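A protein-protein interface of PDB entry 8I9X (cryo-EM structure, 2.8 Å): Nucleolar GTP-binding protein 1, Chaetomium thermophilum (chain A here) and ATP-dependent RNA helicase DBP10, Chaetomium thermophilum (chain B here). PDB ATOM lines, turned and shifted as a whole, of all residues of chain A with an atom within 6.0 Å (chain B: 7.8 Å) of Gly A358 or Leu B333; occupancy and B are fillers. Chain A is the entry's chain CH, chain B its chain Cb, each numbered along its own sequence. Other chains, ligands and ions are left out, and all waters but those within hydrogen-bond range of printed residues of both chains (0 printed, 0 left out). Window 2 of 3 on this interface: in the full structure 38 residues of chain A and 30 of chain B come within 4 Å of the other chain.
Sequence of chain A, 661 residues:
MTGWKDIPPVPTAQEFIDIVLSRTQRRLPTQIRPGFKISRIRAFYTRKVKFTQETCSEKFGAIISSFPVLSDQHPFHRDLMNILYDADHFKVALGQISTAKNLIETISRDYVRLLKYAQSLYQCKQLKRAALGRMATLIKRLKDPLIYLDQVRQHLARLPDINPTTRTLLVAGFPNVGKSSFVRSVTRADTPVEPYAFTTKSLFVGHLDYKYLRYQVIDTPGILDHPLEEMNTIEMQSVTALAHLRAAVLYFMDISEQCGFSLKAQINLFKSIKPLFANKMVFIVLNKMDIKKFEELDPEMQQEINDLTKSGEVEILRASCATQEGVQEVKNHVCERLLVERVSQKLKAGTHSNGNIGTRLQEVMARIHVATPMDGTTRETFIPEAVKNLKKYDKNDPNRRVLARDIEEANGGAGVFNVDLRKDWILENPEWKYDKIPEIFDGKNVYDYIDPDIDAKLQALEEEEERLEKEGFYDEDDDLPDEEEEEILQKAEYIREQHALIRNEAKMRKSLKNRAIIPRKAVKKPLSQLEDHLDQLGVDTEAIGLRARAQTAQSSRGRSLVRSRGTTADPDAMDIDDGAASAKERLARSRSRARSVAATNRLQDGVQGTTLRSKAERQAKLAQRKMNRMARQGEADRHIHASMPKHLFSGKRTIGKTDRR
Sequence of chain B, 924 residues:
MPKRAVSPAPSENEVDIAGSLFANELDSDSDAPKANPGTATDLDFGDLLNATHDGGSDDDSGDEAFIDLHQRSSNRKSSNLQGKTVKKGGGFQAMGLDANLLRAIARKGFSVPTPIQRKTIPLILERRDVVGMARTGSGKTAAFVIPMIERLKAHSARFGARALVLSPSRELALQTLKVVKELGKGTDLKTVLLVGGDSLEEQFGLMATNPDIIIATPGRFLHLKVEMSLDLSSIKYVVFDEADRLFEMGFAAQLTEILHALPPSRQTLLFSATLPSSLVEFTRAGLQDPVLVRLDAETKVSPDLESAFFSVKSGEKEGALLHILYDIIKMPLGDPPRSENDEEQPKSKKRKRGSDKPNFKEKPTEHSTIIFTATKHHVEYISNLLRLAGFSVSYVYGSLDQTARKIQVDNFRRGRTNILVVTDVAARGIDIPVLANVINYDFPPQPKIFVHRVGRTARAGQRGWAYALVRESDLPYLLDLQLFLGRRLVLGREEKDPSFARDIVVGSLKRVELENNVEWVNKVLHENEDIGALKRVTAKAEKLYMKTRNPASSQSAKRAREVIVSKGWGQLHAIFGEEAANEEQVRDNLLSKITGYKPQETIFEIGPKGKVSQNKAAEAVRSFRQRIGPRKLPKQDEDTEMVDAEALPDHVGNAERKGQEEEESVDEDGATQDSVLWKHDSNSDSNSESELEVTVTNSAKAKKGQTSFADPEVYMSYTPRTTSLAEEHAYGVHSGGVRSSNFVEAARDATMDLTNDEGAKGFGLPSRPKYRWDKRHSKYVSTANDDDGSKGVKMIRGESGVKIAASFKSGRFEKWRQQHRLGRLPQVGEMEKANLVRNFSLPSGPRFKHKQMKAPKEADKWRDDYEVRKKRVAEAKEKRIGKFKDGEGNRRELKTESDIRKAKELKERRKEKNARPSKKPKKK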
ATOM      1  N   GLY A 350      -8.596  -5.742   5.885  1.00  0.00           N
ATOM      2  CA  GLY A 350      -8.332  -6.287   4.565  1.00  0.00           C
ATOM      3  C   GLY A 350      -9.296  -5.784   3.511  1.00  0.00           C
ATOM      4  O   GLY A 350      -8.898  -5.545   2.366  1.00  0.00           O
ATOM      5  N   HIS A 352     -10.767  -3.039   1.931  1.00  0.00           N
ATOM      6  CA  HIS A 352     -10.553  -1.603   1.848  1.00  0.00           C
ATOM      7  C   HIS A 352     -11.748  -0.906   1.207  1.00  0.00           C
ATOM      8  O   HIS A 352     -12.638  -1.536   0.629  1.00  0.00           O
ATOM      9  CB  HIS A 352      -9.278  -1.293   1.061  1.00  0.00           C
ATOM     10  CG  HIS A 352      -8.050  -1.935   1.624  1.00  0.00           C
ATOM     11  ND1 HIS A 352      -7.209  -2.725   0.872  1.00  0.00           N
ATOM     12  CD2 HIS A 352      -7.515  -1.897   2.869  1.00  0.00           C
ATOM     13  CE1 HIS A 352      -6.213  -3.151   1.628  1.00  0.00           C
ATOM     14  NE2 HIS A 352      -6.376  -2.662   2.845  1.00  0.00           N
ATOM     15  N   ASN A 356     -10.826  -3.349  -3.555  1.00  0.00           N
ATOM     16  CA  ASN A 356      -9.812  -4.290  -4.013  1.00  0.00           C
ATOM     17  C   ASN A 356      -9.370  -5.195  -2.871  1.00  0.00           C
ATOM     18  O   ASN A 356      -8.951  -4.713  -1.813  1.00  0.00           O
ATOM     19  CB  ASN A 356      -8.614  -3.543  -4.600  1.00  0.00           C
ATOM     20  CG  ASN A 356      -9.019  -2.517  -5.639  1.00  0.00           C
ATOM     21  OD1 ASN A 356     -10.106  -2.594  -6.213  1.00  0.00           O
ATOM     22  ND2 ASN A 356      -8.147  -1.548  -5.887  1.00  0.00           N
ATOM     23  N   ILE A 357      -9.467  -6.507  -3.076  1.00  0.00           N
ATOM     24  CA  ILE A 357      -9.094  -7.460  -2.039  1.00  0.00           C
ATOM     25  C   ILE A 357      -7.576  -7.526  -1.932  1.00  0.00           C
ATOM     26  O   ILE A 357      -6.871  -7.664  -2.940  1.00  0.00           O
ATOM     27  CB  ILE A 357      -9.697  -8.839  -2.340  1.00  0.00           C
ATOM     28  CG1 ILE A 357     -11.225  -8.765  -2.316  1.00  0.00           C
ATOM     29  CG2 ILE A 357      -9.213  -9.855  -1.336  1.00  0.00           C
ATOM     30  CD1 ILE A 357     -11.791  -8.344  -0.978  1.00  0.00           C
ATOM     31  N   GLY A 358      -7.069  -7.426  -0.707  1.00  0.00           N
ATOM     32  CA  GLY A 358      -5.639  -7.434  -0.488  1.00  0.00           C
ATOM     33  C   GLY A 358      -5.005  -8.780  -0.788  1.00  0.00           C
ATOM     34  O   GLY A 358      -5.648  -9.830  -0.784  1.00  0.00           O
ATOM     35  N   THR A 359      -3.699  -8.731  -1.057  1.00  0.00           N
ATOM     36  CA  THR A 359      -2.961  -9.941  -1.402  1.00  0.00           C
ATOM     37  C   THR A 359      -2.951 -10.933  -0.245  1.00  0.00           C
ATOM     38  O   THR A 359      -3.143 -12.138  -0.444  1.00  0.00           O
ATOM     39  CB  THR A 359      -1.533  -9.585  -1.816  1.00  0.00           C
ATOM     40  OG1 THR A 359      -0.747  -9.318  -0.648  1.00  0.00           O
ATOM     41  CG2 THR A 359      -1.530  -8.358  -2.714  1.00  0.00           C
ATOM     42  N   ARG A 360      -2.733 -10.444   0.977  1.00  0.00           N
ATOM     43  CA  ARG A 360      -2.687 -11.341   2.126  1.00  0.00           C
ATOM     44  C   ARG A 360      -4.061 -11.926   2.423  1.00  0.00           C
ATOM     45  O   ARG A 360      -4.179 -13.084   2.840  1.00  0.00           O
ATOM     46  CB  ARG A 360      -2.130 -10.609   3.345  1.00  0.00           C
ATOM     47  CG  ARG A 360      -0.649 -10.302   3.239  1.00  0.00           C
ATOM     48  CD  ARG A 360      -0.205  -9.352   4.329  1.00  0.00           C
ATOM     49  NE  ARG A 360      -0.233  -9.980   5.645  1.00  0.00           N
ATOM     50  CZ  ARG A 360       0.793 -10.616   6.193  1.00  0.00           C
ATOM     51  NH1 ARG A 360       1.946 -10.743   5.558  1.00  0.00           N
ATOM     52  NH2 ARG A 360       0.661 -11.132   7.412  1.00  0.00           N
ATOM     53  N   LEU A 361      -5.118 -11.138   2.220  1.00  0.00           N
ATOM     54  CA  LEU A 361      -6.458 -11.666   2.444  1.00  0.00           C
ATOM     55  C   LEU A 361      -6.794 -12.713   1.390  1.00  0.00           C
ATOM     56  O   LEU A 361      -7.436 -13.726   1.685  1.00  0.00           O
ATOM     57  CB  LEU A 361      -7.485 -10.530   2.458  1.00  0.00           C
ATOM     58  CG  LEU A 361      -8.930 -10.859   2.867  1.00  0.00           C
ATOM     59  CD1 LEU A 361      -9.593  -9.619   3.449  1.00  0.00           C
ATOM     60  CD2 LEU A 361      -9.781 -11.423   1.740  1.00  0.00           C
ATOM     61  N   GLN A 362      -6.343 -12.498   0.150  1.00  0.00           N
ATOM     62  CA  GLN A 362      -6.480 -13.533  -0.870  1.00  0.00           C
ATOM     63  C   GLN A 362      -5.734 -14.796  -0.465  1.00  0.00           C
ATOM     64  O   GLN A 362      -6.240 -15.913  -0.637  1.00  0.00           O
ATOM     65  CB  GLN A 362      -5.961 -13.025  -2.217  1.00  0.00           C
ATOM     66  CG  GLN A 362      -6.810 -11.945  -2.857  1.00  0.00           C
ATOM     67  CD  GLN A 362      -6.166 -11.358  -4.098  1.00  0.00           C
ATOM     68  OE1 GLN A 362      -5.025 -11.678  -4.428  1.00  0.00           O
ATOM     69  NE2 GLN A 362      -6.897 -10.493  -4.792  1.00  0.00           N
ATOM     70  N   GLU A 363      -4.525 -14.636   0.073  1.00  0.00           N
ATOM     71  CA  GLU A 363      -3.737 -15.790   0.495  1.00  0.00           C
ATOM     72  C   GLU A 363      -4.452 -16.570   1.591  1.00  0.00           C
ATOM     73  O   GLU A 363      -4.518 -17.802   1.548  1.00  0.00           O
ATOM     74  CB  GLU A 363      -2.359 -15.337   0.972  1.00  0.00           C
ATOM     75  CG  GLU A 363      -1.400 -14.965  -0.146  1.00  0.00           C
ATOM     76  CD  GLU A 363      -0.535 -13.769   0.203  1.00  0.00           C
ATOM     77  OE1 GLU A 363      -0.243 -13.576   1.402  1.00  0.00           O
ATOM     78  OE2 GLU A 363      -0.147 -13.024  -0.721  1.00  0.00           O
ATOM     79  N   TYR B 326      -1.715   3.516   3.033  1.00  0.00           N
ATOM     80  CA  TYR B 326      -2.994   2.814   3.061  1.00  0.00           C
ATOM     81  C   TYR B 326      -4.159   3.750   3.357  1.00  0.00           C
ATOM     82  O   TYR B 326      -5.199   3.685   2.692  1.00  0.00           O
ATOM     83  CB  TYR B 326      -2.952   1.688   4.097  1.00  0.00           C
ATOM     84  CG  TYR B 326      -2.445   0.368   3.563  1.00  0.00           C
ATOM     85  CD1 TYR B 326      -3.019  -0.217   2.442  1.00  0.00           C
ATOM     86  CD2 TYR B 326      -1.399  -0.299   4.186  1.00  0.00           C
ATOM     87  CE1 TYR B 326      -2.560  -1.425   1.953  1.00  0.00           C
ATOM     88  CE2 TYR B 326      -0.933  -1.508   3.704  1.00  0.00           C
ATOM     89  CZ  TYR B 326      -1.518  -2.066   2.588  1.00  0.00           C
ATOM     90  OH  TYR B 326      -1.058  -3.269   2.105  1.00  0.00           O
ATOM     91  N   LYS B 330      -4.705   6.439   0.101  1.00  0.00           N
ATOM     92  CA  LYS B 330      -5.657   5.442  -0.404  1.00  0.00           C
ATOM     93  C   LYS B 330      -5.102   4.729  -1.643  1.00  0.00           C
ATOM     94  O   LYS B 330      -5.663   4.767  -2.740  1.00  0.00           O
ATOM     95  CB  LYS B 330      -7.048   6.057  -0.649  1.00  0.00           C
ATOM     96  CG  LYS B 330      -7.181   7.129  -1.731  1.00  0.00           C
ATOM     97  CD  LYS B 330      -8.615   7.615  -1.862  1.00  0.00           C
ATOM     98  CE  LYS B 330      -9.011   8.493  -0.686  1.00  0.00           C
ATOM     99  NZ  LYS B 330     -10.367   9.082  -0.864  1.00  0.00           N
ATOM    100  N   MET B 331      -3.985   4.052  -1.428  1.00  0.00           N
ATOM    101  CA  MET B 331      -3.283   3.388  -2.517  1.00  0.00           C
ATOM    102  C   MET B 331      -3.951   2.060  -2.859  1.00  0.00           C
ATOM    103  O   MET B 331      -4.067   1.189  -1.990  1.00  0.00           O
ATOM    104  CB  MET B 331      -1.831   3.149  -2.124  1.00  0.00           C
ATOM    105  CG  MET B 331      -0.922   4.339  -2.305  1.00  0.00           C
ATOM    106  SD  MET B 331      -0.757   4.756  -4.043  1.00  0.00           S
ATOM    107  CE  MET B 331       0.712   3.821  -4.437  1.00  0.00           C
ATOM    108  N   PRO B 332      -4.396   1.864  -4.098  1.00  0.00           N
ATOM    109  CA  PRO B 332      -4.875   0.539  -4.504  1.00  0.00           C
ATOM    110  C   PRO B 332      -3.729  -0.459  -4.547  1.00  0.00           C
ATOM    111  O   PRO B 332      -2.579  -0.102  -4.809  1.00  0.00           O
ATOM    112  CB  PRO B 332      -5.463   0.786  -5.897  1.00  0.00           C
ATOM    113  CG  PRO B 332      -4.732   1.983  -6.400  1.00  0.00           C
ATOM    114  CD  PRO B 332      -4.460   2.840  -5.196  1.00  0.00           C
ATOM    115  N   LEU B 333      -4.053  -1.723  -4.289  1.00  0.00           N
ATOM    116  CA  LEU B 333      -3.059  -2.785  -4.282  1.00  0.00           C
ATOM    117  C   LEU B 333      -3.102  -3.549  -5.600  1.00  0.00           C
ATOM    118  O   LEU B 333      -4.125  -3.551  -6.292  1.00  0.00           O
ATOM    119  CB  LEU B 333      -3.292  -3.738  -3.111  1.00  0.00           C
ATOM    120  CG  LEU B 333      -2.984  -3.181  -1.721  1.00  0.00           C
ATOM    121  CD1 LEU B 333      -3.777  -3.924  -0.661  1.00  0.00           C
ATOM    122  CD2 LEU B 333      -1.492  -3.253  -1.430  1.00  0.00           C
ATOM    123  N   GLY B 334      -1.990  -4.190  -5.942  1.00  0.00           N
ATOM    124  CA  GLY B 334      -1.896  -4.988  -7.148  1.00  0.00           C
ATOM    125  C   GLY B 334      -1.367  -4.190  -8.323  1.00  0.00           C
ATOM    126  O   GLY B 334      -1.096  -2.988  -8.242  1.00  0.00           O
ATOM    127  N   ASP B 335      -1.220  -4.892  -9.438  1.00  0.00           N
ATOM    128  CA  ASP B 335      -0.753  -4.268 -10.669  1.00  0.00           C
ATOM    129  C   ASP B 335      -1.799  -3.288 -11.184  1.00  0.00           C
ATOM    130  O   ASP B 335      -2.984  -3.642 -11.250  1.00  0.00           O
ATOM    131  CB  ASP B 335      -0.452  -5.329 -11.723  1.00  0.00           C
ATOM    132  CG  ASP B 335       0.722  -6.210 -11.346  1.00  0.00           C
ATOM    133  OD1 ASP B 335       1.641  -5.716 -10.660  1.00  0.00           O
ATOM    134  OD2 ASP B 335       0.727  -7.396 -11.735  1.00  0.00           O
ATOM    135  N   PRO B 336      -1.423  -2.063 -11.541  1.00  0.00           N
ATOM    136  CA  PRO B 336      -2.402  -1.102 -12.067  1.00  0.00           C
ATOM    137  C   PRO B 336      -3.019  -1.607 -13.359  1.00  0.00           C
ATOM    138  O   PRO B 336      -2.345  -2.267 -14.163  1.00  0.00           O
ATOM    139  CB  PRO B 336      -1.577   0.172 -12.306  1.00  0.00           C
ATOM    140  CG  PRO B 336      -0.150  -0.225 -12.201  1.00  0.00           C
ATOM    141  CD  PRO B 336      -0.058  -1.516 -11.463  1.00  0.00           C
ATOM    142  N   PRO B 337      -4.307  -1.315 -13.597  1.00  0.00           N
ATOM    143  CA  PRO B 337      -4.997  -1.765 -14.812  1.00  0.00           C
ATOM    144  C   PRO B 337      -4.525  -1.023 -16.058  1.00  0.00           C
ATOM    145  O   PRO B 337      -3.845  -0.006 -15.927  1.00  0.00           O
ATOM    146  CB  PRO B 337      -6.470  -1.459 -14.525  1.00  0.00           C
ATOM    147  CG  PRO B 337      -6.468  -0.434 -13.453  1.00  0.00           C
ATOM    148  CD  PRO B 337      -5.176  -0.530 -12.704  1.00  0.00           C
ATOM    149  N   LEU B 386       7.332  -3.236   0.758  1.00  0.00           N
ATOM    150  CA  LEU B 386       6.127  -2.824   0.047  1.00  0.00           C
ATOM    151  C   LEU B 386       5.685  -3.884  -0.955  1.00  0.00           C
ATOM    152  O   LEU B 386       4.482  -4.087  -1.161  1.00  0.00           O
ATOM    153  CB  LEU B 386       6.356  -1.482  -0.642  1.00  0.00           C
ATOM    154  CG  LEU B 386       6.578  -0.299   0.297  1.00  0.00           C
ATOM    155  CD1 LEU B 386       6.933   0.956  -0.483  1.00  0.00           C
ATOM    156  CD2 LEU B 386       5.346  -0.081   1.155  1.00  0.00           C
ATOM    157  N   ARG B 387       6.639  -4.570  -1.590  1.00  0.00           N
ATOM    158  CA  ARG B 387       6.277  -5.654  -2.496  1.00  0.00           C
ATOM    159  C   ARG B 387       5.601  -6.791  -1.741  1.00  0.00           C
ATOM    160  O   ARG B 387       4.645  -7.396  -2.240  1.00  0.00           O
ATOM    161  CB  ARG B 387       7.516  -6.154  -3.237  1.00  0.00           C
ATOM    162  CG  ARG B 387       7.231  -7.250  -4.250  1.00  0.00           C
ATOM    163  CD  ARG B 387       6.364  -6.726  -5.383  1.00  0.00           C
ATOM    164  NE  ARG B 387       7.000  -5.622  -6.091  1.00  0.00           N
ATOM    165  CZ  ARG B 387       7.880  -5.767  -7.071  1.00  0.00           C
ATOM    166  NH1 ARG B 387       8.250  -6.964  -7.497  1.00  0.00           N
ATOM    167  NH2 ARG B 387       8.401  -4.684  -7.641  1.00  0.00           N
ATOM    168  N   LEU B 388       6.087  -7.097  -0.536  1.00  0.00           N
ATOM    169  CA  LEU B 388       5.398  -8.067   0.311  1.00  0.00           C
ATOM    170  C   LEU B 388       4.000  -7.593   0.673  1.00  0.00           C
ATOM    171  O   LEU B 388       3.055  -8.389   0.669  1.00  0.00           O
ATOM    172  CB  LEU B 388       6.195  -8.329   1.585  1.00  0.00           C
ATOM    173  CG  LEU B 388       7.554  -9.010   1.465  1.00  0.00           C
ATOM    174  CD1 LEU B 388       8.206  -9.034   2.828  1.00  0.00           C
ATOM    175  CD2 LEU B 388       7.409 -10.416   0.907  1.00  0.00           C
ATOM    176  N   ALA B 389       3.853  -6.309   0.998  1.00  0.00           N
ATOM    177  CA  ALA B 389       2.541  -5.737   1.266  1.00  0.00           C
ATOM    178  C   ALA B 389       1.617  -5.793   0.057  1.00  0.00           C
ATOM    179  O   ALA B 389       0.395  -5.778   0.231  1.00  0.00           O
ATOM    180  CB  ALA B 389       2.684  -4.288   1.737  1.00  0.00           C
ATOM    181  N   GLY B 390       2.169  -5.857  -1.152  1.00  0.00           N
ATOM    182  CA  GLY B 390       1.377  -5.998  -2.356  1.00  0.00           C
ATOM    183  C   GLY B 390       1.355  -4.799  -3.277  1.00  0.00           C
ATOM    184  O   GLY B 390       0.579  -4.797  -4.239  1.00  0.00           O
ATOM    185  N   PHE B 391       2.172  -3.784  -3.022  1.00  0.00           N
ATOM    186  CA  PHE B 391       2.165  -2.567  -3.817  1.00  0.00           C
ATOM    187  C   PHE B 391       2.963  -2.761  -5.102  1.00  0.00           C
ATOM    188  O   PHE B 391       3.851  -3.613  -5.183  1.00  0.00           O
ATOM    189  CB  PHE B 391       2.750  -1.404  -3.016  1.00  0.00           C
ATOM    190  CG  PHE B 391       1.828  -0.881  -1.953  1.00  0.00           C
ATOM    191  CD1 PHE B 391       0.745  -0.091  -2.281  1.00  0.00           C
ATOM    192  CD2 PHE B 391       2.056  -1.178  -0.619  1.00  0.00           C
ATOM    193  CE1 PHE B 391      -0.101   0.387  -1.302  1.00  0.00           C
ATOM    194  CE2 PHE B 391       1.214  -0.699   0.365  1.00  0.00           C
ATOM    195  CZ  PHE B 391       0.134   0.085   0.023  1.00  0.00           C
ATOM    196  N   SER B 392       2.632  -1.960  -6.112  1.00  0.00           N
ATOM    197  CA  SER B 392       3.374  -1.941  -7.369  1.00  0.00           C
ATOM    198  C   SER B 392       4.564  -1.006  -7.195  1.00  0.00           C
ATOM    199  O   SER B 392       4.405   0.220  -7.204  1.00  0.00           O
ATOM    200  CB  SER B 392       2.484  -1.489  -8.522  1.00  0.00           C
ATOM    201  OG  SER B 392       1.899  -0.228  -8.251  1.00  0.00           O
ATOM    202  N   ASN B 418       3.394   2.287  -9.133  1.00  0.00           N
ATOM    203  CA  ASN B 418       2.912   3.471  -8.431  1.00  0.00           C
ATOM    204  C   ASN B 418       3.900   3.988  -7.394  1.00  0.00           C
ATOM    205  O   ASN B 418       3.984   5.208  -7.182  1.00  0.00           O
ATOM    206  CB  ASN B 418       1.573   3.165  -7.757  1.00  0.00           C
ATOM    207  CG  ASN B 418       0.445   3.005  -8.752  1.00  0.00           C
ATOM    208  OD1 ASN B 418       0.408   3.680  -9.779  1.00  0.00           O
ATOM    209  ND2 ASN B 418      -0.483   2.104  -8.453  1.00  0.00           N
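Printed residues of chain B within 4 Å of Asn A356: Pro B332.
Gly A358 touches just one residue of chain B: Leu B333.
Printed residues of chain A within 4 Å of Leu B333: His A352 and Gly A358.
Printed residues of chain A within 4 Å of Gly B390: Thr A359.
Asn B418 touches none of the printed residues of chain A.
The nearest residue of chain B that does not touch Gly A358 is Ala B389 (6.3 Å).
The nearest residue of chain A that does not touch Leu B333 is Asn A356 (4.4 Å).
The nearest printed residue of chain B that does not touch Thr A359 is Leu B388 (4.1 Å).
Hydrophobic or aromatic side chains of chain B that line the printed part of chain A: Pro B332 and Leu B333.
Among the printed residues, no Asp or Glu carboxylate lies within 4 Å of a Lys or Arg side-chain nitrogen of the other chain.
The backbone carbonyl oxygen of Ala B389 lies within hydrogen-bond range of the side-chain hydroxyl of Tyr B326 (3.5 Å).
The backbone NH of Gly B334 is in hydrogen-bond range of the backbone carbonyl oxygen of Gly B390.
Among the printed residues, pairs that only touch across the chains: His A352 with Leu B333 (3.4 Å), Asn A356 with Pro B332 (3.6 Å), Gly A358 with Leu B333 (3.98 Å), Thr A359 with Ala B389 (3.8 Å) and Thr A359 with Gly B390 (3.8 Å).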
